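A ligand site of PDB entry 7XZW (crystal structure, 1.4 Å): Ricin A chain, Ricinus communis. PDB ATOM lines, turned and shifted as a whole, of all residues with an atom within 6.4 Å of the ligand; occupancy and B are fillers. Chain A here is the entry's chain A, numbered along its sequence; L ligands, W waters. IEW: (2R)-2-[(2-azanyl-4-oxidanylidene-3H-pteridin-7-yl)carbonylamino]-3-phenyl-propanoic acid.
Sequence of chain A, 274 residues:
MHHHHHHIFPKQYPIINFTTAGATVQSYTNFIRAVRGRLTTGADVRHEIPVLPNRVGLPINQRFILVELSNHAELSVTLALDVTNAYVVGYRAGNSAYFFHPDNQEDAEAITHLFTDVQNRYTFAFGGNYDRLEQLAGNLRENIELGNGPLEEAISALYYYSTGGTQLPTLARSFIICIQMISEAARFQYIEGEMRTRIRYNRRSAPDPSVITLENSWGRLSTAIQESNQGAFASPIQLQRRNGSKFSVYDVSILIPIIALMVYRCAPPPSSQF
Water W3 lies within hydrogen-bond range of an oxygen (OAQ) of the ligand (2.8 Å), the backbone NH of Asp 131 (3.0 Å) and the backbone NH of Tyr 130 (3.4 Å).
Water W1 lies within hydrogen-bond range of N of the ligand (2.9 Å) and OD1 of Asn 216 (3.0 Å).
Water W2 lies within hydrogen-bond range of O of Glu 215, OE2 of Glu 184 and N of the ligand.
Water W4 lies within hydrogen-bond range of the side-chain hydroxyl (OH) of Tyr 87 (3.0 Å) and a nitrogen (N) of the ligand (3.5 Å).
Ala 86 touches the ligand.
Tyr 87 touches the ligand (CE2 to C8A, 3.3 Å).
Phe 100 touches the ligand (CE2 to N2, 3.6 Å).
CA of Asn 129 touches OAQ of the ligand, 3.7 Å away.
Ile 179 touches the ligand (CG2 to C4, 3.4 Å).
OE2 of Glu 184 touches C6 of the ligand, 3.8 Å away.
Hydrophobic or aromatic side chains within 4 Å of the ligand: Tyr 87, Val 88, Phe 100, Tyr 130 and Ile 179.
Of the 19 residues printed, 11 come within 4 Å of the ligand.
The nearest printed residue that does not touch the ligand is Glu 215 (4.5 Å).
The side-chain carboxylate (OE1) of Glu 184 lies within salt-bridge range of the guanidinium group (NH1) of Arg 187, 3.1 Å away.
The guanidinium group (NH2) of Arg 187 lies within hydrogen-bond range of the backbone carbonyl oxygen (O) of Asn 85.
OG of Ser 183 sits at hydrogen-bond distance from O of Ala 86 (2.7 Å).
The side-chain amide oxygen (OD1) of Asn 85 lies within hydrogen-bond range of the backbone NH (N) of Tyr 87, at 3.0 Å.
N of Phe 100 sits at hydrogen-bond distance from O of Val 89 (3.1 Å).
The side-chain hydroxyl of Tyr 130 sits at hydrogen-bond distance from the side-chain carboxylate of Glu 184, at 2.6 Å.
N of Glu 184 lies within hydrogen-bond range of O of Ile 179.
The guanidinium group of Arg 187 is in hydrogen-bond range of an oxygen (O4) of the ligand (2.8 Å).
The backbone carbonyl oxygen of Gly 128 lies within hydrogen-bond range of a nitrogen (N2) of the ligand (3.1 Å).
OG of Ser 183 lies close to O4 of the ligand.
O of Val 88 sits at hydrogen-bond distance from N2 of the ligand, at 2.9 Å.
An oxygen (OAQ) of the ligand lies within hydrogen-bond range of the backbone NH (N) of Tyr 130 (2.9 Å).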
ATOM      1  N   ASN A  85      20.827  -3.392   4.455  1.00  0.00           N
ATOM      2  CA  ASN A  85      21.130  -4.417   5.454  1.00  0.00           C
ATOM      3  C   ASN A  85      20.680  -4.086   6.876  1.00  0.00           C
ATOM      4  O   ASN A  85      20.914  -4.881   7.799  1.00  0.00           O
ATOM      5  CB  ASN A  85      22.628  -4.761   5.423  1.00  0.00           C
ATOM      6  CG  ASN A  85      23.524  -3.543   5.586  1.00  0.00           C
ATOM      7  OD1 ASN A  85      23.084  -2.477   6.033  1.00  0.00           O
ATOM      8  ND2 ASN A  85      24.786  -3.686   5.223  1.00  0.00           N
ATOM      9  N   ALA A  86      20.032  -2.926   7.043  1.00  0.00           N
ATOM     10  CA  ALA A  86      19.634  -2.383   8.349  1.00  0.00           C
ATOM     11  C   ALA A  86      20.802  -2.061   9.298  1.00  0.00           C
ATOM     12  O   ALA A  86      20.595  -1.813  10.484  1.00  0.00           O
ATOM     13  CB  ALA A  86      18.574  -3.259   9.033  1.00  0.00           C
ATOM     14  N   TYR A  87      22.034  -2.038   8.771  1.00  0.00           N
ATOM     15  CA  TYR A  87      23.212  -1.741   9.593  1.00  0.00           C
ATOM     16  C   TYR A  87      23.246  -0.299  10.077  1.00  0.00           C
ATOM     17  O   TYR A  87      22.940   0.625   9.326  1.00  0.00           O
ATOM     18  CB  TYR A  87      24.514  -2.073   8.852  1.00  0.00           C
ATOM     19  CG  TYR A  87      25.009  -3.508   9.039  1.00  0.00           C
ATOM     20  CD1 TYR A  87      24.180  -4.593   8.735  1.00  0.00           C
ATOM     21  CD2 TYR A  87      26.296  -3.769   9.500  1.00  0.00           C
ATOM     22  CE1 TYR A  87      24.616  -5.899   8.894  1.00  0.00           C
ATOM     23  CE2 TYR A  87      26.748  -5.078   9.664  1.00  0.00           C
ATOM     24  CZ  TYR A  87      25.898  -6.145   9.364  1.00  0.00           C
ATOM     25  OH  TYR A  87      26.311  -7.453   9.513  1.00  0.00           O
ATOM     26  N   VAL A  88      23.599  -0.137  11.354  1.00  0.00           N
ATOM     27  CA  VAL A  88      23.883   1.177  11.905  1.00  0.00           C
ATOM     28  C   VAL A  88      25.264   1.574  11.385  1.00  0.00           C
ATOM     29  O   VAL A  88      26.264   0.943  11.721  1.00  0.00           O
ATOM     30  CB  VAL A  88      23.855   1.156  13.451  1.00  0.00           C
ATOM     31  CG1 VAL A  88      24.222   2.512  14.020  1.00  0.00           C
ATOM     32  CG2 VAL A  88      22.492   0.714  13.962  1.00  0.00           C
ATOM     33  N   VAL A  89      25.317   2.608  10.543  1.00  0.00           N
ATOM     34  CA  VAL A  89      26.577   3.019   9.911  1.00  0.00           C
ATOM     35  C   VAL A  89      27.285   4.151  10.660  1.00  0.00           C
ATOM     36  O   VAL A  89      28.469   4.402  10.454  1.00  0.00           O
ATOM     37  CB  VAL A  89      26.415   3.366   8.408  1.00  0.00           C
ATOM     38  CG1 VAL A  89      25.870   2.169   7.637  1.00  0.00           C
ATOM     39  CG2 VAL A  89      25.543   4.603   8.199  1.00  0.00           C
ATOM     40  N   PHE A 100      31.348   4.326  11.518  1.00  0.00           N
ATOM     41  CA  PHE A 100      32.199   3.139  11.513  1.00  0.00           C
ATOM     42  C   PHE A 100      33.052   3.121  10.246  1.00  0.00           C
ATOM     43  O   PHE A 100      32.651   3.660   9.212  1.00  0.00           O
ATOM     44  CB  PHE A 100      31.384   1.859  11.635  1.00  0.00           C
ATOM     45  CG  PHE A 100      30.602   1.757  12.913  1.00  0.00           C
ATOM     46  CD1 PHE A 100      31.265   1.652  14.148  1.00  0.00           C
ATOM     47  CD2 PHE A 100      29.206   1.729  12.906  1.00  0.00           C
ATOM     48  CE1 PHE A 100      30.550   1.553  15.334  1.00  0.00           C
ATOM     49  CE2 PHE A 100      28.490   1.629  14.092  1.00  0.00           C
ATOM     50  CZ  PHE A 100      29.154   1.542  15.313  1.00  0.00           C
ATOM     51  N   GLY A 128      32.159  -1.665  12.460  1.00  0.00           N
ATOM     52  CA  GLY A 128      31.020  -1.722  13.362  1.00  0.00           C
ATOM     53  C   GLY A 128      30.382  -3.081  13.586  1.00  0.00           C
ATOM     54  O   GLY A 128      29.288  -3.146  14.155  1.00  0.00           O
ATOM     55  N   ASN A 129      31.045  -4.152  13.139  1.00  0.00           N
ATOM     56  CA  ASN A 129      30.596  -5.529  13.340  1.00  0.00           C
ATOM     57  C   ASN A 129      30.668  -5.939  14.817  1.00  0.00           C
ATOM     58  O   ASN A 129      31.453  -5.363  15.583  1.00  0.00           O
ATOM     59  CB  ASN A 129      31.418  -6.493  12.488  1.00  0.00           C
ATOM     60  CG  ASN A 129      32.919  -6.267  12.612  1.00  0.00           C
ATOM     61  OD1 ASN A 129      33.466  -5.322  12.047  1.00  0.00           O
ATOM     62  ND2 ASN A 129      33.582  -7.132  13.363  1.00  0.00           N
ATOM     63  N   TYR A 130      29.854  -6.925  15.207  1.00  0.00           N
ATOM     64  CA  TYR A 130      29.841  -7.411  16.603  1.00  0.00           C
ATOM     65  C   TYR A 130      31.210  -7.856  17.105  1.00  0.00           C
ATOM     66  O   TYR A 130      31.577  -7.484  18.221  1.00  0.00           O
ATOM     67  CB  TYR A 130      28.845  -8.557  16.799  1.00  0.00           C
ATOM     68  CG  TYR A 130      27.380  -8.182  16.727  1.00  0.00           C
ATOM     69  CD1 TYR A 130      26.875  -7.025  17.358  1.00  0.00           C
ATOM     70  CD2 TYR A 130      26.485  -9.014  16.057  1.00  0.00           C
ATOM     71  CE1 TYR A 130      25.517  -6.710  17.291  1.00  0.00           C
ATOM     72  CE2 TYR A 130      25.135  -8.700  15.984  1.00  0.00           C
ATOM     73  CZ  TYR A 130      24.668  -7.561  16.598  1.00  0.00           C
ATOM     74  OH  TYR A 130      23.324  -7.282  16.519  1.00  0.00           O
ATOM     75  N   ASP A 131      31.944  -8.618  16.297  1.00  0.00           N
ATOM     76  CA  ASP A 131      33.289  -9.102  16.648  1.00  0.00           C
ATOM     77  C   ASP A 131      34.194  -7.974  17.164  1.00  0.00           C
ATOM     78  O   ASP A 131      34.765  -8.079  18.260  1.00  0.00           O
ATOM     79  CB  ASP A 131      33.956  -9.820  15.465  1.00  0.00           C
ATOM     80  CG  ASP A 131      33.511 -11.275  15.302  1.00  0.00           C
ATOM     81  OD1 ASP A 131      32.836 -11.829  16.196  1.00  0.00           O
ATOM     82  OD2 ASP A 131      33.852 -11.875  14.256  1.00  0.00           O
ATOM     83  N   LEU A 133      33.203  -4.817  17.985  1.00  0.00           N
ATOM     84  CA  LEU A 133      32.580  -4.079  19.080  1.00  0.00           C
ATOM     85  C   LEU A 133      32.676  -4.803  20.411  1.00  0.00           C
ATOM     86  O   LEU A 133      32.891  -4.164  21.446  1.00  0.00           O
ATOM     87  CB  LEU A 133      31.116  -3.716  18.747  1.00  0.00           C
ATOM     88  CG  LEU A 133      30.861  -2.700  17.620  1.00  0.00           C
ATOM     89  CD1 LEU A 133      29.357  -2.557  17.449  1.00  0.00           C
ATOM     90  CD2 LEU A 133      31.503  -1.339  17.865  1.00  0.00           C
ATOM     91  N   ARG A 141      28.246 -10.236  23.488  1.00  0.00           N
ATOM     92  CA  ARG A 141      26.794 -10.008  23.514  1.00  0.00           C
ATOM     93  C   ARG A 141      26.076 -10.796  24.614  1.00  0.00           C
ATOM     94  O   ARG A 141      25.187 -10.261  25.263  1.00  0.00           O
ATOM     95  CB  ARG A 141      26.178 -10.333  22.148  1.00  0.00           C
ATOM     96  CG  ARG A 141      26.358  -9.264  21.085  1.00  0.00           C
ATOM     97  CD  ARG A 141      25.963  -9.820  19.725  1.00  0.00           C
ATOM     98  NE  ARG A 141      26.988 -10.715  19.173  1.00  0.00           N
ATOM     99  CZ  ARG A 141      26.785 -11.648  18.255  1.00  0.00           C
ATOM    100  NH1 ARG A 141      25.576 -11.855  17.749  1.00  0.00           N
ATOM    101  NH2 ARG A 141      27.800 -12.378  17.824  1.00  0.00           N
ATOM    102  N   ILE A 179      22.177  -1.574  18.347  1.00  0.00           N
ATOM    103  CA  ILE A 179      22.099  -2.445  17.171  1.00  0.00           C
ATOM    104  C   ILE A 179      21.078  -3.568  17.385  1.00  0.00           C
ATOM    105  O   ILE A 179      20.251  -3.846  16.511  1.00  0.00           O
ATOM    106  CB  ILE A 179      23.485  -2.999  16.770  1.00  0.00           C
ATOM    107  CG1 ILE A 179      24.376  -1.865  16.233  1.00  0.00           C
ATOM    108  CG2 ILE A 179      23.370  -4.100  15.730  1.00  0.00           C
ATOM    109  CD1 ILE A 179      25.860  -2.152  16.324  1.00  0.00           C
ATOM    110  N   SER A 183      18.129  -2.625  14.969  1.00  0.00           N
ATOM    111  CA  SER A 183      18.364  -3.384  13.741  1.00  0.00           C
ATOM    112  C   SER A 183      17.953  -4.860  13.836  1.00  0.00           C
ATOM    113  O   SER A 183      17.228  -5.357  12.967  1.00  0.00           O
ATOM    114  CB  SER A 183      19.822  -3.258  13.307  1.00  0.00           C
ATOM    115  OG  SER A 183      20.163  -1.894  13.164  1.00  0.00           O
ATOM    116  N   GLU A 184      18.381  -5.545  14.891  1.00  0.00           N
ATOM    117  CA  GLU A 184      18.016  -6.963  15.039  1.00  0.00           C
ATOM    118  C   GLU A 184      16.535  -7.174  15.279  1.00  0.00           C
ATOM    119  O   GLU A 184      15.949  -8.127  14.761  1.00  0.00           O
ATOM    120  CB  GLU A 184      18.831  -7.683  16.119  1.00  0.00           C
ATOM    121  CG  GLU A 184      20.345  -7.651  15.924  1.00  0.00           C
ATOM    122  CD  GLU A 184      20.865  -8.478  14.758  1.00  0.00           C
ATOM    123  OE1 GLU A 184      20.082  -9.001  13.930  1.00  0.00           O
ATOM    124  OE2 GLU A 184      22.106  -8.599  14.665  1.00  0.00           O
ATOM    125  N   ARG A 187      14.889  -6.873  11.979  1.00  0.00           N
ATOM    126  CA  ARG A 187      15.138  -8.080  11.171  1.00  0.00           C
ATOM    127  C   ARG A 187      14.320  -9.286  11.627  1.00  0.00           C
ATOM    128  O   ARG A 187      13.901 -10.096  10.791  1.00  0.00           O
ATOM    129  CB  ARG A 187      16.612  -8.459  11.207  1.00  0.00           C
ATOM    130  CG  ARG A 187      17.549  -7.503  10.498  1.00  0.00           C
ATOM    131  CD  ARG A 187      18.988  -7.843  10.848  1.00  0.00           C
ATOM    132  NE  ARG A 187      19.894  -6.823  10.333  1.00  0.00           N
ATOM    133  CZ  ARG A 187      20.938  -6.330  10.991  1.00  0.00           C
ATOM    134  NH1 ARG A 187      21.239  -6.747  12.227  1.00  0.00           N
ATOM    135  NH2 ARG A 187      21.693  -5.409  10.424  1.00  0.00           N
ATOM    136  N   GLU A 215      20.872 -13.777  15.330  1.00  0.00           N
ATOM    137  CA  GLU A 215      21.734 -12.661  14.898  1.00  0.00           C
ATOM    138  C   GLU A 215      22.880 -13.159  14.025  1.00  0.00           C
ATOM    139  O   GLU A 215      23.112 -12.625  12.950  1.00  0.00           O
ATOM    140  CB  GLU A 215      22.296 -11.897  16.091  1.00  0.00           C
ATOM    141  CG  GLU A 215      21.240 -11.205  16.924  1.00  0.00           C
ATOM    142  CD  GLU A 215      21.796 -10.596  18.193  1.00  0.00           C
ATOM    143  OE1 GLU A 215      22.996 -10.775  18.486  1.00  0.00           O
ATOM    144  OE2 GLU A 215      21.014  -9.928  18.902  1.00  0.00           O
ATOM    145  N   ASN A 216      23.565 -14.203  14.501  1.00  0.00           N
ATOM    146  CA  ASN A 216      24.711 -14.753  13.784  1.00  0.00           C
ATOM    147  C   ASN A 216      24.347 -15.390  12.449  1.00  0.00           C
ATOM    148  O   ASN A 216      25.184 -15.453  11.551  1.00  0.00           O
ATOM    149  CB  ASN A 216      25.461 -15.758  14.659  1.00  0.00           C
ATOM    150  CG  ASN A 216      26.164 -15.100  15.837  1.00  0.00           C
ATOM    151  OD1 ASN A 216      26.391 -13.888  15.860  1.00  0.00           O
ATOM    152  ND2 ASN A 216      26.529 -15.917  16.823  1.00  0.00           N
ATOM    153  N   TRP A 218      21.681 -14.479  10.353  1.00  0.00           N
ATOM    154  CA  TRP A 218      20.795 -13.687   9.494  1.00  0.00           C
ATOM    155  C   TRP A 218      21.149 -13.777   8.012  1.00  0.00           C
ATOM    156  O   TRP A 218      20.258 -14.009   7.186  1.00  0.00           O
ATOM    157  CB  TRP A 218      20.729 -12.224   9.937  1.00  0.00           C
ATOM    158  CG  TRP A 218      19.732 -11.398   9.162  1.00  0.00           C
ATOM    159  CD1 TRP A 218      18.388 -11.639   9.024  1.00  0.00           C
ATOM    160  CD2 TRP A 218      19.995 -10.183   8.439  1.00  0.00           C
ATOM    161  NE1 TRP A 218      17.799 -10.655   8.263  1.00  0.00           N
ATOM    162  CE2 TRP A 218      18.763  -9.758   7.882  1.00  0.00           C
ATOM    163  CE3 TRP A 218      21.150  -9.418   8.211  1.00  0.00           C
ATOM    164  CZ2 TRP A 218      18.648  -8.586   7.116  1.00  0.00           C
ATOM    165  CZ3 TRP A 218      21.045  -8.254   7.442  1.00  0.00           C
ATOM    166  CH2 TRP A 218      19.792  -7.851   6.907  1.00  0.00           C
HETATM  167  C2  IEW L   1      26.243  -2.618  12.940  1.00  0.00           C
HETATM  168  C4  IEW L   1      24.186  -3.794  12.489  1.00  0.00           C
HETATM  169  C6  IEW L   1      25.024  -7.383  12.602  1.00  0.00           C
HETATM  170  C7  IEW L   1      26.389  -7.324  12.880  1.00  0.00           C
HETATM  171  O4  IEW L   1      22.976  -3.759  12.250  1.00  0.00           O
HETATM  172  N   IEW L   1      26.552  -9.660  12.709  1.00  0.00           N
HETATM  173  CAL IEW L   1      27.158  -8.495  12.995  1.00  0.00           C
HETATM  174  OAQ IEW L   1      28.370  -8.436  13.278  1.00  0.00           O
HETATM  175  N8  IEW L   1      26.967  -6.112  13.024  1.00  0.00           N
HETATM  176  C8A IEW L   1      26.264  -4.974  12.910  1.00  0.00           C
HETATM  177  N1  IEW L   1      26.887  -3.799  13.062  1.00  0.00           N
HETATM  178  N2  IEW L   1      26.906  -1.485  13.094  1.00  0.00           N
HETATM  179  N3  IEW L   1      24.877  -2.595  12.657  1.00  0.00           N
HETATM  180  C4A IEW L   1      24.889  -5.007  12.620  1.00  0.00           C
HETATM  181  N5  IEW L   1      24.278  -6.193  12.483  1.00  0.00           N
HETATM  182  O   HOH W   1      27.638 -12.179  13.788  1.00  0.00           O
HETATM  183  O   HOH W   2      23.148  -9.965  12.478  1.00  0.00           O
HETATM  184  O   HOH W   3      30.802  -9.816  13.800  1.00  0.00           O
HETATM  185  O   HOH W   4      24.365  -9.631  10.003  1.00  0.00           O
